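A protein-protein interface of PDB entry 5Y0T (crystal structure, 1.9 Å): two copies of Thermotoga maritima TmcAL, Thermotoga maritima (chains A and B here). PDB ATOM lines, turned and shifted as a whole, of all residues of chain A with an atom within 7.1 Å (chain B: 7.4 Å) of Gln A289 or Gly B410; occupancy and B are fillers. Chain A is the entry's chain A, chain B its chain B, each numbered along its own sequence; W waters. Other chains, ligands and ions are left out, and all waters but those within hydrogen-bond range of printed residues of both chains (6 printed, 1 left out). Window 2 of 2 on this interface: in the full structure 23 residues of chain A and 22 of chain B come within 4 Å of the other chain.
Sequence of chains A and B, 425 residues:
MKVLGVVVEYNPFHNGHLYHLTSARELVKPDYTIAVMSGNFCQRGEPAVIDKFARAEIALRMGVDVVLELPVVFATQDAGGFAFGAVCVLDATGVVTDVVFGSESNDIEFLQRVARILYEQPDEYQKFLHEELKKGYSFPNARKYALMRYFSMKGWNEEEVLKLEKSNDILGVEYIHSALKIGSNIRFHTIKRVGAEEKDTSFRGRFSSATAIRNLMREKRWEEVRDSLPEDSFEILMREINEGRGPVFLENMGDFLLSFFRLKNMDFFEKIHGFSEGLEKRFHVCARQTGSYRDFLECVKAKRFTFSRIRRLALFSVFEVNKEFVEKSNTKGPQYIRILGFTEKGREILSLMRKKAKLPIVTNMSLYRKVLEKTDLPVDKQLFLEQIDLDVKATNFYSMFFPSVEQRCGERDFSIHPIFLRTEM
Of the 14 printed residues of chain A, 5 touch a printed residue of chain B. Of the 12 printed residues of chain B, 5 touch a printed residue of chain A. Printed residues of chain B that touch a printed residue of chain A: Asn B396, Arg B408, CME B409, Gly B410 and Glu B411. Among the printed residues, no Asp or Glu carboxylate lies within 4 Å of a Lys or Arg side-chain nitrogen of the other chain.
N of Gly B410 sits at hydrogen-bond distance from O of Arg A288, at 2.9 Å. The backbone carbonyl oxygen of Gln A289 lies close to SG of CME B409. The guanidinium group of Arg A262 is in hydrogen-bond range of the backbone carbonyl oxygen of Arg B408. The backbone carbonyl oxygen (O) of Asn B396 sits at hydrogen-bond distance from the guanidinium group (NH1) of Arg A262, at 3.0 Å. The backbone NH (N) of Gly A291 lies within hydrogen-bond range of SG of CME B409 (3.3 Å).
Among the printed residues, merely in contact across the chains: Arg A288 with Glu B411 (3.8 Å), Gln A289 with Gly B410 (3.9 Å), Thr A290 with CME B409 (3.7 Å) and Gly A291 with Arg B408 (3.9 Å).
Water W1 lies within hydrogen-bond range of OD2 of Asp A295 (2.6 Å), N of Gly A291 (2.8 Å) and SG of CME B409 (3.3 Å). Water W5 lies within hydrogen-bond range of O of Arg A262 (2.6 Å), ND2 of Asn B396 (2.9 Å) and NH2 of Arg A288 (3.3 Å). Water W4 bridges the backbone carbonyl oxygen of Gly A291 (2.7 Å) and the guanidinium group of Arg B408 (2.8 Å). Water W2 lies within hydrogen-bond range of OE2 of Glu B411 and NE of Arg A288. Water W3 lies within hydrogen-bond range of the side-chain amide nitrogen (NE2) of Gln A289 and the side-chain carboxylate (OE1) of Glu B411. Water W6 lies within hydrogen-bond range of N of Glu B411 (2.8 Å) and NE2 of Gln A289 (3.0 Å).
The backbone carbonyl oxygen (O) of Glu B411 is in hydrogen-bond range of the side-chain hydroxyl (OG) of Ser B415 (3.5 Å). The backbone carbonyl oxygen (O) of Arg A262 sits at hydrogen-bond distance from the guanidinium group (NH2) of Arg A288, at 3.4 Å. The side-chain carboxylate (OE2) of Glu B411 sits at hydrogen-bond distance from the side-chain amide nitrogen (ND2) of Asn B396 (2.8 Å). The backbone carbonyl oxygen (O) of Cys A286 sits at hydrogen-bond distance from the side-chain hydroxyl (OG1) of Thr A290. NH2 of Arg A262 lies within hydrogen-bond range of O of Thr A290. SG of Cys A286 is disulfide-bonded to SG of Cys A299, 2.1 Å away.
Of the printed residues of chain B, Arg A288 touches Gly B410 and Glu B411. Of chain B, only CME B409 and Gly B410 come within 4 Å of Gln A289. Of the printed residues of chain A, Asn B396 touches Arg A262. Of the printed residues of chain A, Arg B408 touches Arg A262 (2.6 Å) and Gly A291 (3.9 Å). Of the printed residues of chain A, CME B409 touches Gln A289 (3.4 Å), Thr A290 (3.7 Å) and Gly A291 (3.3 Å). Of chain A, only Arg A288 and Gln A289 come within 4 Å of Gly B410. Arg B412 touches none of the printed residues of chain A. The nearest printed residue of chain B that does not touch Thr A290 is Arg B408 (4.1 Å).
No position is printed for both chains. Of the 9 pairs that touch across the chains among the printed residues, none has its exchanged pair printed and touching as well.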
ATOM      1  N   LEU A 258     -22.533  10.962  23.424  1.00  0.00           N
ATOM      2  CA  LEU A 258     -21.533  10.138  22.776  1.00  0.00           C
ATOM      3  C   LEU A 258     -22.107   9.517  21.501  1.00  0.00           C
ATOM      4  O   LEU A 258     -21.446   9.508  20.452  1.00  0.00           O
ATOM      5  CB  LEU A 258     -21.014   9.059  23.736  1.00  0.00           C
ATOM      6  CG  LEU A 258     -19.995   8.077  23.134  1.00  0.00           C
ATOM      7  CD1 LEU A 258     -18.815   8.837  22.537  1.00  0.00           C
ATOM      8  CD2 LEU A 258     -19.504   7.072  24.180  1.00  0.00           C
ATOM      9  N   ARG A 262     -21.212  10.158  17.218  1.00  0.00           N
ATOM     10  CA  ARG A 262     -20.906   9.117  16.236  1.00  0.00           C
ATOM     11  C   ARG A 262     -21.728   9.259  14.963  1.00  0.00           C
ATOM     12  O   ARG A 262     -21.508   8.542  13.984  1.00  0.00           O
ATOM     13  CB  ARG A 262     -21.141   7.723  16.822  1.00  0.00           C
ATOM     14  CG  ARG A 262     -20.190   7.343  17.932  1.00  0.00           C
ATOM     15  CD  ARG A 262     -20.373   5.891  18.337  1.00  0.00           C
ATOM     16  NE  ARG A 262     -19.350   5.488  19.293  1.00  0.00           N
ATOM     17  CZ  ARG A 262     -19.157   4.247  19.714  1.00  0.00           C
ATOM     18  NH1 ARG A 262     -19.911   3.258  19.251  1.00  0.00           N
ATOM     19  NH2 ARG A 262     -18.182   3.989  20.583  1.00  0.00           N
ATOM     20  N   PHE A 283     -12.854  15.286  18.734  1.00  0.00           N
ATOM     21  CA  PHE A 283     -14.246  14.887  18.957  1.00  0.00           C
ATOM     22  C   PHE A 283     -14.590  13.688  18.073  1.00  0.00           C
ATOM     23  O   PHE A 283     -15.181  12.722  18.536  1.00  0.00           O
ATOM     24  CB  PHE A 283     -15.227  16.037  18.671  1.00  0.00           C
ATOM     25  CG  PHE A 283     -15.712  16.757  19.904  1.00  0.00           C
ATOM     26  CD1 PHE A 283     -14.814  17.404  20.740  1.00  0.00           C
ATOM     27  CD2 PHE A 283     -17.071  16.801  20.223  1.00  0.00           C
ATOM     28  CE1 PHE A 283     -15.248  18.084  21.872  1.00  0.00           C
ATOM     29  CE2 PHE A 283     -17.518  17.482  21.356  1.00  0.00           C
ATOM     30  CZ  PHE A 283     -16.612  18.117  22.186  1.00  0.00           C
ATOM     31  N   HIS A 284     -14.189  13.750  16.808  1.00  0.00           N
ATOM     32  CA  HIS A 284     -14.538  12.711  15.845  1.00  0.00           C
ATOM     33  C   HIS A 284     -13.937  11.359  16.214  1.00  0.00           C
ATOM     34  O   HIS A 284     -14.633  10.333  16.216  1.00  0.00           O
ATOM     35  CB  HIS A 284     -14.084  13.122  14.445  1.00  0.00           C
ATOM     36  CG  HIS A 284     -14.560  12.202  13.361  1.00  0.00           C
ATOM     37  ND1 HIS A 284     -13.792  11.168  12.872  1.00  0.00           N
ATOM     38  CD2 HIS A 284     -15.730  12.159  12.679  1.00  0.00           C
ATOM     39  CE1 HIS A 284     -14.464  10.530  11.929  1.00  0.00           C
ATOM     40  NE2 HIS A 284     -15.642  11.115  11.790  1.00  0.00           N
ATOM     41  N   VAL A 285     -12.639  11.363  16.518  1.00  0.00           N
ATOM     42  CA  VAL A 285     -11.919  10.138  16.848  1.00  0.00           C
ATOM     43  C   VAL A 285     -12.342   9.588  18.210  1.00  0.00           C
ATOM     44  O   VAL A 285     -12.634   8.404  18.332  1.00  0.00           O
ATOM     45  CB  VAL A 285     -10.389  10.364  16.832  1.00  0.00           C
ATOM     46  CG1 VAL A 285      -9.644   9.086  17.219  1.00  0.00           C
ATOM     47  CG2 VAL A 285      -9.935  10.833  15.456  1.00  0.00           C
ATOM     48  N   CYS A 286     -12.395  10.447  19.229  1.00  0.00           N
ATOM     49  CA  CYS A 286     -12.719   9.974  20.573  1.00  0.00           C
ATOM     50  C   CYS A 286     -14.138   9.430  20.673  1.00  0.00           C
ATOM     51  O   CYS A 286     -14.401   8.508  21.449  1.00  0.00           O
ATOM     52  CB  CYS A 286     -12.518  11.087  21.606  1.00  0.00           C
ATOM     53  SG  CYS A 286     -10.763  11.489  21.851  1.00  0.00           S
ATOM     54  N   ALA A 287     -15.051   9.994  19.889  1.00  0.00           N
ATOM     55  CA  ALA A 287     -16.437   9.518  19.895  1.00  0.00           C
ATOM     56  C   ALA A 287     -16.514   8.067  19.420  1.00  0.00           C
ATOM     57  O   ALA A 287     -17.314   7.275  19.916  1.00  0.00           O
ATOM     58  CB  ALA A 287     -17.310  10.405  19.020  1.00  0.00           C
ATOM     59  N   ARG A 288     -15.692   7.737  18.439  1.00  0.00           N
ATOM     60  CA  ARG A 288     -15.682   6.392  17.873  1.00  0.00           C
ATOM     61  C   ARG A 288     -14.837   5.395  18.667  1.00  0.00           C
ATOM     62  O   ARG A 288     -15.078   4.184  18.611  1.00  0.00           O
ATOM     63  CB  ARG A 288     -15.226   6.460  16.414  1.00  0.00           C
ATOM     64  CG  ARG A 288     -16.307   7.052  15.515  1.00  0.00           C
ATOM     65  CD  ARG A 288     -15.744   7.792  14.308  1.00  0.00           C
ATOM     66  NE  ARG A 288     -16.829   8.333  13.492  1.00  0.00           N
ATOM     67  CZ  ARG A 288     -17.533   9.425  13.793  1.00  0.00           C
ATOM     68  NH1 ARG A 288     -17.269  10.118  14.895  1.00  0.00           N
ATOM     69  NH2 ARG A 288     -18.512   9.827  12.987  1.00  0.00           N
ATOM     70  N   GLN A 289     -13.830   5.889  19.383  1.00  0.00           N
ATOM     71  CA  GLN A 289     -12.937   4.998  20.118  1.00  0.00           C
ATOM     72  C   GLN A 289     -13.289   4.771  21.597  1.00  0.00           C
ATOM     73  O   GLN A 289     -12.755   3.851  22.223  1.00  0.00           O
ATOM     74  CB  GLN A 289     -11.510   5.519  20.002  1.00  0.00           C
ATOM     75  CG  GLN A 289     -10.973   5.427  18.584  1.00  0.00           C
ATOM     76  CD  GLN A 289     -11.114   4.026  17.987  1.00  0.00           C
ATOM     77  OE1 GLN A 289     -10.828   3.018  18.644  1.00  0.00           O
ATOM     78  NE2 GLN A 289     -11.553   3.961  16.733  1.00  0.00           N
ATOM     79  N   THR A 290     -14.209   5.564  22.145  1.00  0.00           N
ATOM     80  CA  THR A 290     -14.599   5.395  23.542  1.00  0.00           C
ATOM     81  C   THR A 290     -16.043   4.905  23.653  1.00  0.00           C
ATOM     82  O   THR A 290     -16.836   5.071  22.727  1.00  0.00           O
ATOM     83  CB  THR A 290     -14.441   6.711  24.366  1.00  0.00           C
ATOM     84  OG1 THR A 290     -15.312   7.727  23.848  1.00  0.00           O
ATOM     85  CG2 THR A 290     -12.989   7.191  24.343  1.00  0.00           C
ATOM     86  N   GLY A 291     -16.353   4.250  24.770  1.00  0.00           N
ATOM     87  CA  GLY A 291     -17.665   3.674  25.004  1.00  0.00           C
ATOM     88  C   GLY A 291     -18.524   4.358  26.054  1.00  0.00           C
ATOM     89  O   GLY A 291     -19.654   3.936  26.285  1.00  0.00           O
ATOM     90  N   SER A 292     -17.987   5.387  26.706  1.00  0.00           N
ATOM     91  CA  SER A 292     -18.768   6.191  27.647  1.00  0.00           C
ATOM     92  C   SER A 292     -18.328   7.635  27.555  1.00  0.00           C
ATOM     93  O   SER A 292     -17.188   7.921  27.188  1.00  0.00           O
ATOM     94  CB  SER A 292     -18.606   5.698  29.087  1.00  0.00           C
ATOM     95  OG  SER A 292     -17.331   6.065  29.600  1.00  0.00           O
ATOM     96  N   ASP A 295     -15.290   8.446  29.484  1.00  0.00           N
ATOM     97  CA  ASP A 295     -14.066   8.090  28.767  1.00  0.00           C
ATOM     98  C   ASP A 295     -13.841   9.040  27.591  1.00  0.00           C
ATOM     99  O   ASP A 295     -12.698   9.399  27.291  1.00  0.00           O
ATOM    100  CB  ASP A 295     -14.108   6.639  28.276  1.00  0.00           C
ATOM    101  CG  ASP A 295     -14.021   5.631  29.414  1.00  0.00           C
ATOM    102  OD1 ASP A 295     -13.699   6.035  30.553  1.00  0.00           O
ATOM    103  OD2 ASP A 295     -14.271   4.431  29.168  1.00  0.00           O
ATOM    104  N   CYS A 299     -10.533  11.231  26.818  1.00  0.00           N
ATOM    105  CA  CYS A 299      -9.847  11.071  25.541  1.00  0.00           C
ATOM    106  C   CYS A 299      -9.602  12.417  24.851  1.00  0.00           C
ATOM    107  O   CYS A 299      -8.526  12.650  24.310  1.00  0.00           O
ATOM    108  CB  CYS A 299     -10.643  10.141  24.613  1.00  0.00           C
ATOM    109  SG  CYS A 299      -9.945   9.952  22.941  1.00  0.00           S
ATOM    110  N   THR B 395     -23.412   1.069  11.874  1.00  0.00           N
ATOM    111  CA  THR B 395     -22.711   0.135  12.750  1.00  0.00           C
ATOM    112  C   THR B 395     -22.243   0.797  14.042  1.00  0.00           C
ATOM    113  O   THR B 395     -22.397   0.240  15.134  1.00  0.00           O
ATOM    114  CB  THR B 395     -21.476  -0.469  12.063  1.00  0.00           C
ATOM    115  OG1 THR B 395     -21.861  -1.071  10.820  1.00  0.00           O
ATOM    116  CG2 THR B 395     -20.809  -1.511  12.968  1.00  0.00           C
ATOM    117  N   ASN B 396     -21.629   1.967  13.905  1.00  0.00           N
ATOM    118  CA  ASN B 396     -21.116   2.695  15.056  1.00  0.00           C
ATOM    119  C   ASN B 396     -22.238   3.139  16.010  1.00  0.00           C
ATOM    120  O   ASN B 396     -22.086   3.105  17.242  1.00  0.00           O
ATOM    121  CB  ASN B 396     -20.310   3.909  14.595  1.00  0.00           C
ATOM    122  CG  ASN B 396     -18.984   3.520  13.929  1.00  0.00           C
ATOM    123  OD1 ASN B 396     -18.509   2.387  14.055  1.00  0.00           O
ATOM    124  ND2 ASN B 396     -18.376   4.472  13.238  1.00  0.00           N
ATOM    125  N   SER B 399     -23.674   0.028  17.900  1.00  0.00           N
ATOM    126  CA  SER B 399     -22.776  -0.565  18.887  1.00  0.00           C
ATOM    127  C   SER B 399     -22.850   0.109  20.248  1.00  0.00           C
ATOM    128  O   SER B 399     -22.492  -0.492  21.260  1.00  0.00           O
ATOM    129  CB  SER B 399     -21.329  -0.534  18.369  1.00  0.00           C
ATOM    130  OG  SER B 399     -21.168  -1.506  17.344  1.00  0.00           O
ATOM    131  N   GLN B 407     -18.258  -3.362  25.380  1.00  0.00           N
ATOM    132  CA  GLN B 407     -18.327  -3.742  23.971  1.00  0.00           C
ATOM    133  C   GLN B 407     -18.588  -2.561  23.035  1.00  0.00           C
ATOM    134  O   GLN B 407     -18.695  -2.750  21.824  1.00  0.00           O
ATOM    135  CB  GLN B 407     -19.415  -4.807  23.767  1.00  0.00           C
ATOM    136  CG  GLN B 407     -19.089  -6.145  24.422  1.00  0.00           C
ATOM    137  CD  GLN B 407     -17.885  -6.795  23.794  1.00  0.00           C
ATOM    138  OE1 GLN B 407     -17.864  -7.049  22.593  1.00  0.00           O
ATOM    139  NE2 GLN B 407     -16.865  -7.057  24.601  1.00  0.00           N
ATOM    140  N   ARG B 408     -18.684  -1.349  23.585  1.00  0.00           N
ATOM    141  CA  ARG B 408     -19.161  -0.198  22.807  1.00  0.00           C
ATOM    142  C   ARG B 408     -18.071   0.614  22.088  1.00  0.00           C
ATOM    143  O   ARG B 408     -18.375   1.503  21.297  1.00  0.00           O
ATOM    144  CB  ARG B 408     -19.969   0.732  23.722  1.00  0.00           C
ATOM    145  CG  ARG B 408     -21.206   0.059  24.308  1.00  0.00           C
ATOM    146  CD  ARG B 408     -21.940   0.937  25.325  1.00  0.00           C
ATOM    147  NE  ARG B 408     -23.159   0.265  25.775  1.00  0.00           N
ATOM    148  CZ  ARG B 408     -24.035   0.773  26.634  1.00  0.00           C
ATOM    149  NH1 ARG B 408     -23.839   1.975  27.166  1.00  0.00           N
ATOM    150  NH2 ARG B 408     -25.109   0.072  26.962  1.00  0.00           N
ATOM    151  N   CME B 409     -16.808   0.310  22.358  1.00  0.00           N
ATOM    152  CA  CME B 409     -15.697   1.056  21.781  1.00  0.00           C
ATOM    153  CB  CME B 409     -14.394   0.927  22.572  1.00  0.00           C
ATOM    154  SG  CME B 409     -14.590   1.554  24.183  1.00  0.00           S
ATOM    155  SD  CME B 409     -15.398   0.054  25.409  1.00  0.00           S
ATOM    156  CE  CME B 409     -14.705   0.318  27.006  1.00  0.00           C
ATOM    157  CZ  CME B 409     -13.192   0.267  27.018  1.00  0.00           C
ATOM    158  OH  CME B 409     -12.829  -0.986  26.455  1.00  0.00           O
ATOM    159  C   CME B 409     -15.286   0.534  20.419  1.00  0.00           C
ATOM    160  O   CME B 409     -15.357  -0.653  20.092  1.00  0.00           O
ATOM    161  N   GLY B 410     -14.817   1.468  19.598  1.00  0.00           N
ATOM    162  CA  GLY B 410     -14.190   1.118  18.334  1.00  0.00           C
ATOM    163  C   GLY B 410     -15.166   1.106  17.174  1.00  0.00           C
ATOM    164  O   GLY B 410     -16.374   1.155  17.376  1.00  0.00           O
ATOM    165  N   GLU B 411     -14.637   1.057  15.953  1.00  0.00           N
ATOM    166  CA  GLU B 411     -15.480   0.941  14.770  1.00  0.00           C
ATOM    167  C   GLU B 411     -15.406  -0.476  14.241  1.00  0.00           C
ATOM    168  O   GLU B 411     -14.396  -0.863  13.654  1.00  0.00           O
ATOM    169  CB  GLU B 411     -15.038   1.924  13.696  1.00  0.00           C
ATOM    170  CG  GLU B 411     -15.062   3.379  14.155  1.00  0.00           C
ATOM    171  CD  GLU B 411     -14.786   4.343  13.019  1.00  0.00           C
ATOM    172  OE1 GLU B 411     -13.637   4.815  12.905  1.00  0.00           O
ATOM    173  OE2 GLU B 411     -15.725   4.631  12.246  1.00  0.00           O
ATOM    174  N   ARG B 412     -16.484  -1.232  14.426  1.00  0.00           N
ATOM    175  CA  ARG B 412     -16.469  -2.668  14.169  1.00  0.00           C
ATOM    176  C   ARG B 412     -16.265  -2.968  12.701  1.00  0.00           C
ATOM    177  O   ARG B 412     -15.730  -4.010  12.355  1.00  0.00           O
ATOM    178  CB  ARG B 412     -17.767  -3.337  14.649  1.00  0.00           C
ATOM    179  CG  ARG B 412     -17.885  -3.473  16.178  1.00  0.00           C
ATOM    180  CD  ARG B 412     -18.942  -4.521  16.566  1.00  0.00           C
ATOM    181  NE  ARG B 412     -18.342  -5.551  17.413  1.00  0.00           N
ATOM    182  CZ  ARG B 412     -18.592  -6.852  17.327  1.00  0.00           C
ATOM    183  NH1 ARG B 412     -19.435  -7.320  16.418  1.00  0.00           N
ATOM    184  NH2 ARG B 412     -17.971  -7.690  18.141  1.00  0.00           N
ATOM    185  N   ASP B 413     -16.714  -2.066  11.835  1.00  0.00           N
ATOM    186  CA  ASP B 413     -16.491  -2.255  10.414  1.00  0.00           C
ATOM    187  C   ASP B 413     -15.002  -2.335  10.092  1.00  0.00           C
ATOM    188  O   ASP B 413     -14.608  -3.041   9.172  1.00  0.00           O
ATOM    189  CB  ASP B 413     -17.122  -1.130   9.600  1.00  0.00           C
ATOM    190  CG  ASP B 413     -18.604  -1.315   9.410  1.00  0.00           C
ATOM    191  OD1 ASP B 413     -19.010  -2.310   8.775  1.00  0.00           O
ATOM    192  OD2 ASP B 413     -19.356  -0.449   9.882  1.00  0.00           O
ATOM    193  N   PHE B 414     -14.190  -1.544  10.787  1.00  0.00           N
ATOM    194  CA  PHE B 414     -12.731  -1.623  10.626  1.00  0.00           C
ATOM    195  C   PHE B 414     -12.029  -2.665  11.499  1.00  0.00           C
ATOM    196  O   PHE B 414     -10.979  -3.171  11.128  1.00  0.00           O
ATOM    197  CB  PHE B 414     -12.124  -0.238  10.854  1.00  0.00           C
ATOM    198  CG  PHE B 414     -12.678   0.797   9.916  1.00  0.00           C
ATOM    199  CD1 PHE B 414     -13.759   1.581  10.284  1.00  0.00           C
ATOM    200  CD2 PHE B 414     -12.159   0.943   8.644  1.00  0.00           C
ATOM    201  CE1 PHE B 414     -14.291   2.518   9.413  1.00  0.00           C
ATOM    202  CE2 PHE B 414     -12.691   1.875   7.768  1.00  0.00           C
ATOM    203  CZ  PHE B 414     -13.759   2.662   8.156  1.00  0.00           C
ATOM    204  N   SER B 415     -12.579  -2.962  12.672  1.00  0.00           N
ATOM    205  CA  SER B 415     -11.907  -3.887  13.590  1.00  0.00           C
ATOM    206  C   SER B 415     -12.226  -5.359  13.329  1.00  0.00           C
ATOM    207  O   SER B 415     -11.469  -6.236  13.736  1.00  0.00           O
ATOM    208  CB  SER B 415     -12.256  -3.542  15.038  1.00  0.00           C
ATOM    209  OG  SER B 415     -13.625  -3.801  15.290  1.00  0.00           O
HETATM  210  O   HOH W   1     -14.405   3.637  26.705  1.00  0.00           O
HETATM  211  O   HOH W   2     -16.522   6.834  10.883  1.00  0.00           O
HETATM  212  O   HOH W   3     -11.987   6.043  15.045  1.00  0.00           O
HETATM  213  O   HOH W   4     -21.808   3.836  27.893  1.00  0.00           O
HETATM  214  O   HOH W   5     -19.862   6.877  12.773  1.00  0.00           O
HETATM  215  O   HOH W   6     -11.816   1.172  15.663  1.00  0.00           O
